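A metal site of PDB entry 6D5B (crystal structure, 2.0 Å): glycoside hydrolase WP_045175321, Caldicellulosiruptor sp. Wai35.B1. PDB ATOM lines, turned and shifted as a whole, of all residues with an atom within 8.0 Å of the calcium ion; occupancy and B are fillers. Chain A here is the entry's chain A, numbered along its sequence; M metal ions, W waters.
The calcium ion is bound by O of Asn 133 (2.3 Å), O of Thr 61 (2.4 Å), OD1 of Asn 136 (2.4 Å), OD2 of Asp 63 (2.5 Å), water W1 (2.5 Å), OG1 of Thr 61 (2.5 Å), OD1 of Asp 137 (2.6 Å) and OD1 of Asp 63 (2.7 Å). The calcium ion has eight donor atoms within binding distance.
OD1 of Asn 133 lies within hydrogen-bond range of OG of Ser 30 (2.9 Å). The backbone carbonyl oxygen (O) of Asp 63 lies within hydrogen-bond range of the side-chain amino group (NZ) of Lys 126. The backbone NH (N) of Gly 135 sits at hydrogen-bond distance from the side-chain amide oxygen (OD1) of Asn 133 (3.1 Å).
Of the 21 residues printed, 5 come within 4 Å of the calcium ion. The nearest printed residue that does not touch the calcium ion is Gln 134 (4.4 Å).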
ATOM      1  N   SER A  30      -2.349 -31.037 -16.092  1.00  0.00           N
ATOM      2  CA  SER A  30      -1.635 -29.981 -15.431  1.00  0.00           C
ATOM      3  C   SER A  30      -0.153 -30.159 -15.614  1.00  0.00           C
ATOM      4  O   SER A  30       0.590 -29.193 -15.882  1.00  0.00           O
ATOM      5  CB  SER A  30      -1.945 -29.927 -13.957  1.00  0.00           C
ATOM      6  OG  SER A  30      -1.385 -28.724 -13.435  1.00  0.00           O
ATOM      7  N   ILE A  35       2.780 -27.129 -23.364  1.00  0.00           N
ATOM      8  CA  ILE A  35       1.605 -26.260 -23.233  1.00  0.00           C
ATOM      9  C   ILE A  35       1.037 -26.030 -24.642  1.00  0.00           C
ATOM     10  O   ILE A  35       1.750 -25.824 -25.583  1.00  0.00           O
ATOM     11  CB  ILE A  35       1.967 -24.947 -22.520  1.00  0.00           C
ATOM     12  CG1 ILE A  35       2.502 -25.287 -21.091  1.00  0.00           C
ATOM     13  CG2 ILE A  35       0.736 -24.053 -22.415  1.00  0.00           C
ATOM     14  CD1 ILE A  35       2.908 -24.128 -20.204  1.00  0.00           C
ATOM     15  N   TRP A  59       0.114 -15.792 -20.416  1.00  0.00           N
ATOM     16  CA  TRP A  59       0.853 -15.503 -19.208  1.00  0.00           C
ATOM     17  C   TRP A  59       0.921 -16.780 -18.419  1.00  0.00           C
ATOM     18  O   TRP A  59      -0.082 -17.527 -18.309  1.00  0.00           O
ATOM     19  CB  TRP A  59       0.140 -14.440 -18.361  1.00  0.00           C
ATOM     20  CG  TRP A  59      -0.138 -13.158 -19.077  1.00  0.00           C
ATOM     21  CD1 TRP A  59      -1.143 -12.945 -19.999  1.00  0.00           C
ATOM     22  CD2 TRP A  59       0.550 -11.930 -18.920  1.00  0.00           C
ATOM     23  NE1 TRP A  59      -1.137 -11.640 -20.375  1.00  0.00           N
ATOM     24  CE2 TRP A  59      -0.057 -11.013 -19.785  1.00  0.00           C
ATOM     25  CE3 TRP A  59       1.664 -11.513 -18.163  1.00  0.00           C
ATOM     26  CZ2 TRP A  59       0.402  -9.693 -19.896  1.00  0.00           C
ATOM     27  CZ3 TRP A  59       2.085 -10.216 -18.275  1.00  0.00           C
ATOM     28  CH2 TRP A  59       1.451  -9.324 -19.121  1.00  0.00           C
ATOM     29  N   TYR A  60       2.093 -17.085 -17.908  1.00  0.00           N
ATOM     30  CA  TYR A  60       2.285 -18.362 -17.209  1.00  0.00           C
ATOM     31  C   TYR A  60       3.537 -18.352 -16.349  1.00  0.00           C
ATOM     32  O   TYR A  60       4.359 -17.406 -16.378  1.00  0.00           O
ATOM     33  CB  TYR A  60       2.302 -19.556 -18.198  1.00  0.00           C
ATOM     34  CG  TYR A  60       3.480 -19.547 -19.085  1.00  0.00           C
ATOM     35  CD1 TYR A  60       3.562 -18.630 -20.134  1.00  0.00           C
ATOM     36  CD2 TYR A  60       4.552 -20.362 -18.836  1.00  0.00           C
ATOM     37  CE1 TYR A  60       4.708 -18.559 -20.902  1.00  0.00           C
ATOM     38  CE2 TYR A  60       5.661 -20.307 -19.626  1.00  0.00           C
ATOM     39  CZ  TYR A  60       5.722 -19.426 -20.677  1.00  0.00           C
ATOM     40  OH  TYR A  60       6.840 -19.369 -21.455  1.00  0.00           O
ATOM     41  N   THR A  61       3.671 -19.425 -15.584  1.00  0.00           N
ATOM     42  CA  THR A  61       4.857 -19.636 -14.806  1.00  0.00           C
ATOM     43  C   THR A  61       5.658 -20.762 -15.466  1.00  0.00           C
ATOM     44  O   THR A  61       5.109 -21.847 -15.707  1.00  0.00           O
ATOM     45  CB  THR A  61       4.540 -19.945 -13.348  1.00  0.00           C
ATOM     46  OG1 THR A  61       3.505 -20.953 -13.235  1.00  0.00           O
ATOM     47  CG2 THR A  61       4.036 -18.688 -12.700  1.00  0.00           C
ATOM     48  N   VAL A  62       6.948 -20.468 -15.708  1.00  0.00           N
ATOM     49  CA  VAL A  62       7.852 -21.356 -16.385  1.00  0.00           C
ATOM     50  C   VAL A  62       8.157 -22.656 -15.592  1.00  0.00           C
ATOM     51  O   VAL A  62       8.421 -23.721 -16.205  1.00  0.00           O
ATOM     52  CB  VAL A  62       9.126 -20.613 -16.818  1.00  0.00           C
ATOM     53  CG1 VAL A  62      10.041 -20.269 -15.625  1.00  0.00           C
ATOM     54  CG2 VAL A  62       9.890 -21.374 -17.916  1.00  0.00           C
ATOM     55  N   ASP A  63       8.066 -22.601 -14.265  1.00  0.00           N
ATOM     56  CA  ASP A  63       8.340 -23.805 -13.418  1.00  0.00           C
ATOM     57  C   ASP A  63       9.744 -24.387 -13.532  1.00  0.00           C
ATOM     58  O   ASP A  63       9.949 -25.583 -13.887  1.00  0.00           O
ATOM     59  CB  ASP A  63       7.335 -24.920 -13.715  1.00  0.00           C
ATOM     60  CG  ASP A  63       5.927 -24.453 -13.714  1.00  0.00           C
ATOM     61  OD1 ASP A  63       5.605 -23.574 -12.877  1.00  0.00           O
ATOM     62  OD2 ASP A  63       5.157 -24.939 -14.568  1.00  0.00           O
ATOM     63  N   GLY A  64      10.718 -23.562 -13.226  1.00  0.00           N
ATOM     64  CA  GLY A  64      12.101 -23.914 -13.560  1.00  0.00           C
ATOM     65  C   GLY A  64      12.511 -23.394 -14.927  1.00  0.00           C
ATOM     66  O   GLY A  64      12.328 -24.069 -15.945  1.00  0.00           O
ATOM     67  N   GLY A  95       0.301 -15.789 -10.957  1.00  0.00           N
ATOM     68  CA  GLY A  95       0.250 -16.790 -12.028  1.00  0.00           C
ATOM     69  C   GLY A  95       1.107 -16.516 -13.267  1.00  0.00           C
ATOM     70  O   GLY A  95       0.940 -17.183 -14.309  1.00  0.00           O
ATOM     71  N   ALA A  96       2.045 -15.585 -13.164  1.00  0.00           N
ATOM     72  CA  ALA A  96       2.967 -15.387 -14.240  1.00  0.00           C
ATOM     73  C   ALA A  96       4.327 -14.835 -13.860  1.00  0.00           C
ATOM     74  O   ALA A  96       4.477 -13.866 -13.071  1.00  0.00           O
ATOM     75  CB  ALA A  96       2.328 -14.519 -15.315  1.00  0.00           C
ATOM     76  N   ASP A  97       5.322 -15.493 -14.423  1.00  0.00           N
ATOM     77  CA  ASP A  97       6.687 -14.943 -14.517  1.00  0.00           C
ATOM     78  C   ASP A  97       7.150 -14.862 -15.964  1.00  0.00           C
ATOM     79  O   ASP A  97       8.266 -14.415 -16.238  1.00  0.00           O
ATOM     80  CB  ASP A  97       7.699 -15.763 -13.649  1.00  0.00           C
ATOM     81  CG  ASP A  97       7.771 -17.250 -14.031  1.00  0.00           C
ATOM     82  OD1 ASP A  97       7.530 -17.660 -15.176  1.00  0.00           O
ATOM     83  OD2 ASP A  97       8.120 -18.066 -13.165  1.00  0.00           O
ATOM     84  N   LYS A 126       9.872 -26.529 -22.847  1.00  0.00           N
ATOM     85  CA  LYS A 126      11.243 -26.188 -22.437  1.00  0.00           C
ATOM     86  C   LYS A 126      12.225 -27.029 -23.234  1.00  0.00           C
ATOM     87  O   LYS A 126      11.902 -28.098 -23.722  1.00  0.00           O
ATOM     88  CB  LYS A 126      11.398 -26.320 -20.940  1.00  0.00           C
ATOM     89  CG  LYS A 126      10.541 -25.284 -20.192  1.00  0.00           C
ATOM     90  CD  LYS A 126      10.564 -25.405 -18.667  1.00  0.00           C
ATOM     91  CE  LYS A 126       9.573 -26.415 -18.100  1.00  0.00           C
ATOM     92  NZ  LYS A 126       9.490 -26.207 -16.625  1.00  0.00           N
ATOM     93  N   ASN A 131       9.075 -30.710 -17.282  1.00  0.00           N
ATOM     94  CA  ASN A 131       7.648 -30.511 -17.131  1.00  0.00           C
ATOM     95  C   ASN A 131       7.302 -29.088 -16.717  1.00  0.00           C
ATOM     96  O   ASN A 131       8.069 -28.401 -16.034  1.00  0.00           O
ATOM     97  CB  ASN A 131       7.061 -31.470 -16.103  1.00  0.00           C
ATOM     98  CG  ASN A 131       6.883 -32.868 -16.663  1.00  0.00           C
ATOM     99  OD1 ASN A 131       6.646 -33.057 -17.862  1.00  0.00           O
ATOM    100  ND2 ASN A 131       7.010 -33.871 -15.783  1.00  0.00           N
ATOM    101  N   TYR A 132       6.156 -28.660 -17.189  1.00  0.00           N
ATOM    102  CA  TYR A 132       5.511 -27.514 -16.666  1.00  0.00           C
ATOM    103  C   TYR A 132       4.465 -28.017 -15.713  1.00  0.00           C
ATOM    104  O   TYR A 132       4.110 -29.187 -15.706  1.00  0.00           O
ATOM    105  CB  TYR A 132       4.789 -26.786 -17.795  1.00  0.00           C
ATOM    106  CG  TYR A 132       5.628 -26.092 -18.820  1.00  0.00           C
ATOM    107  CD1 TYR A 132       6.234 -24.876 -18.559  1.00  0.00           C
ATOM    108  CD2 TYR A 132       5.747 -26.623 -20.096  1.00  0.00           C
ATOM    109  CE1 TYR A 132       6.951 -24.214 -19.525  1.00  0.00           C
ATOM    110  CE2 TYR A 132       6.455 -25.971 -21.090  1.00  0.00           C
ATOM    111  CZ  TYR A 132       7.025 -24.765 -20.834  1.00  0.00           C
ATOM    112  OH  TYR A 132       7.732 -24.130 -21.813  1.00  0.00           O
ATOM    113  N   ASN A 133       3.972 -27.069 -14.935  1.00  0.00           N
ATOM    114  CA  ASN A 133       2.788 -27.192 -14.124  1.00  0.00           C
ATOM    115  C   ASN A 133       1.834 -26.108 -14.594  1.00  0.00           C
ATOM    116  O   ASN A 133       2.088 -24.920 -14.350  1.00  0.00           O
ATOM    117  CB  ASN A 133       3.105 -26.966 -12.630  1.00  0.00           C
ATOM    118  CG  ASN A 133       1.871 -26.872 -11.772  1.00  0.00           C
ATOM    119  OD1 ASN A 133       0.797 -27.274 -12.197  1.00  0.00           O
ATOM    120  ND2 ASN A 133       2.002 -26.340 -10.555  1.00  0.00           N
ATOM    121  N   GLN A 134       0.716 -26.495 -15.199  1.00  0.00           N
ATOM    122  CA  GLN A 134      -0.138 -25.498 -15.826  1.00  0.00           C
ATOM    123  C   GLN A 134      -1.086 -24.890 -14.827  1.00  0.00           C
ATOM    124  O   GLN A 134      -1.621 -23.797 -15.059  1.00  0.00           O
ATOM    125  CB  GLN A 134      -0.906 -26.116 -16.950  1.00  0.00           C
ATOM    126  CG  GLN A 134       0.005 -26.660 -18.019  1.00  0.00           C
ATOM    127  CD  GLN A 134      -0.757 -26.885 -19.254  1.00  0.00           C
ATOM    128  OE1 GLN A 134      -0.925 -25.962 -20.071  1.00  0.00           O
ATOM    129  NE2 GLN A 134      -1.314 -28.081 -19.376  1.00  0.00           N
ATOM    130  N   GLY A 135      -1.284 -25.622 -13.726  1.00  0.00           N
ATOM    131  CA  GLY A 135      -2.157 -25.246 -12.622  1.00  0.00           C
ATOM    132  C   GLY A 135      -1.868 -23.931 -11.944  1.00  0.00           C
ATOM    133  O   GLY A 135      -2.763 -23.294 -11.391  1.00  0.00           O
ATOM    134  N   ASN A 136      -0.630 -23.483 -12.030  1.00  0.00           N
ATOM    135  CA  ASN A 136      -0.243 -22.175 -11.436  1.00  0.00           C
ATOM    136  C   ASN A 136       0.038 -21.146 -12.572  1.00  0.00           C
ATOM    137  O   ASN A 136       0.886 -20.246 -12.444  1.00  0.00           O
ATOM    138  CB  ASN A 136       0.971 -22.372 -10.527  1.00  0.00           C
ATOM    139  CG  ASN A 136       2.143 -22.922 -11.267  1.00  0.00           C
ATOM    140  OD1 ASN A 136       2.075 -23.071 -12.500  1.00  0.00           O
ATOM    141  ND2 ASN A 136       3.233 -23.259 -10.554  1.00  0.00           N
ATOM    142  N   ASP A 137      -0.661 -21.329 -13.684  1.00  0.00           N
ATOM    143  CA  ASP A 137      -0.568 -20.403 -14.864  1.00  0.00           C
ATOM    144  C   ASP A 137      -1.775 -19.502 -14.992  1.00  0.00           C
ATOM    145  O   ASP A 137      -2.914 -20.000 -15.174  1.00  0.00           O
ATOM    146  CB  ASP A 137      -0.462 -21.210 -16.176  1.00  0.00           C
ATOM    147  CG  ASP A 137       0.851 -21.865 -16.290  1.00  0.00           C
ATOM    148  OD1 ASP A 137       1.735 -21.534 -15.456  1.00  0.00           O
ATOM    149  OD2 ASP A 137       1.006 -22.699 -17.200  1.00  0.00           O
ATOM    150  N   TRP A 138      -1.536 -18.190 -14.973  1.00  0.00           N
ATOM    151  CA  TRP A 138      -2.608 -17.192 -15.151  1.00  0.00           C
ATOM    152  C   TRP A 138      -3.552 -17.532 -16.331  1.00  0.00           C
ATOM    153  O   TRP A 138      -4.779 -17.572 -16.181  1.00  0.00           O
ATOM    154  CB  TRP A 138      -2.005 -15.799 -15.341  1.00  0.00           C
ATOM    155  CG  TRP A 138      -3.022 -14.693 -15.583  1.00  0.00           C
ATOM    156  CD1 TRP A 138      -3.340 -14.124 -16.784  1.00  0.00           C
ATOM    157  CD2 TRP A 138      -3.861 -14.092 -14.613  1.00  0.00           C
ATOM    158  NE1 TRP A 138      -4.291 -13.195 -16.597  1.00  0.00           N
ATOM    159  CE2 TRP A 138      -4.614 -13.134 -15.272  1.00  0.00           C
ATOM    160  CE3 TRP A 138      -4.015 -14.246 -13.252  1.00  0.00           C
ATOM    161  CZ2 TRP A 138      -5.572 -12.329 -14.612  1.00  0.00           C
ATOM    162  CZ3 TRP A 138      -4.948 -13.414 -12.574  1.00  0.00           C
ATOM    163  CH2 TRP A 138      -5.708 -12.479 -13.267  1.00  0.00           C
ATOM    164  N   TRP A 140      -3.998 -20.342 -18.103  1.00  0.00           N
ATOM    165  CA  TRP A 140      -4.517 -21.678 -18.354  1.00  0.00           C
ATOM    166  C   TRP A 140      -6.019 -21.810 -18.008  1.00  0.00           C
ATOM    167  O   TRP A 140      -6.500 -21.322 -16.995  1.00  0.00           O
ATOM    168  CB  TRP A 140      -3.696 -22.726 -17.615  1.00  0.00           C
ATOM    169  CG  TRP A 140      -3.916 -24.132 -18.092  1.00  0.00           C
ATOM    170  CD1 TRP A 140      -3.913 -24.539 -19.366  1.00  0.00           C
ATOM    171  CD2 TRP A 140      -4.140 -25.287 -17.290  1.00  0.00           C
ATOM    172  NE1 TRP A 140      -4.118 -25.898 -19.436  1.00  0.00           N
ATOM    173  CE2 TRP A 140      -4.201 -26.396 -18.167  1.00  0.00           C
ATOM    174  CE3 TRP A 140      -4.211 -25.519 -15.919  1.00  0.00           C
ATOM    175  CZ2 TRP A 140      -4.414 -27.697 -17.731  1.00  0.00           C
ATOM    176  CZ3 TRP A 140      -4.378 -26.836 -15.459  1.00  0.00           C
ATOM    177  CH2 TRP A 140      -4.508 -27.907 -16.375  1.00  0.00           C
HETATM  178 CA    CA M   1       3.493 -23.136 -14.487  1.00  0.00          CA
HETATM  179  O   HOH W   1       3.599 -23.813 -16.893  1.00  0.00           O
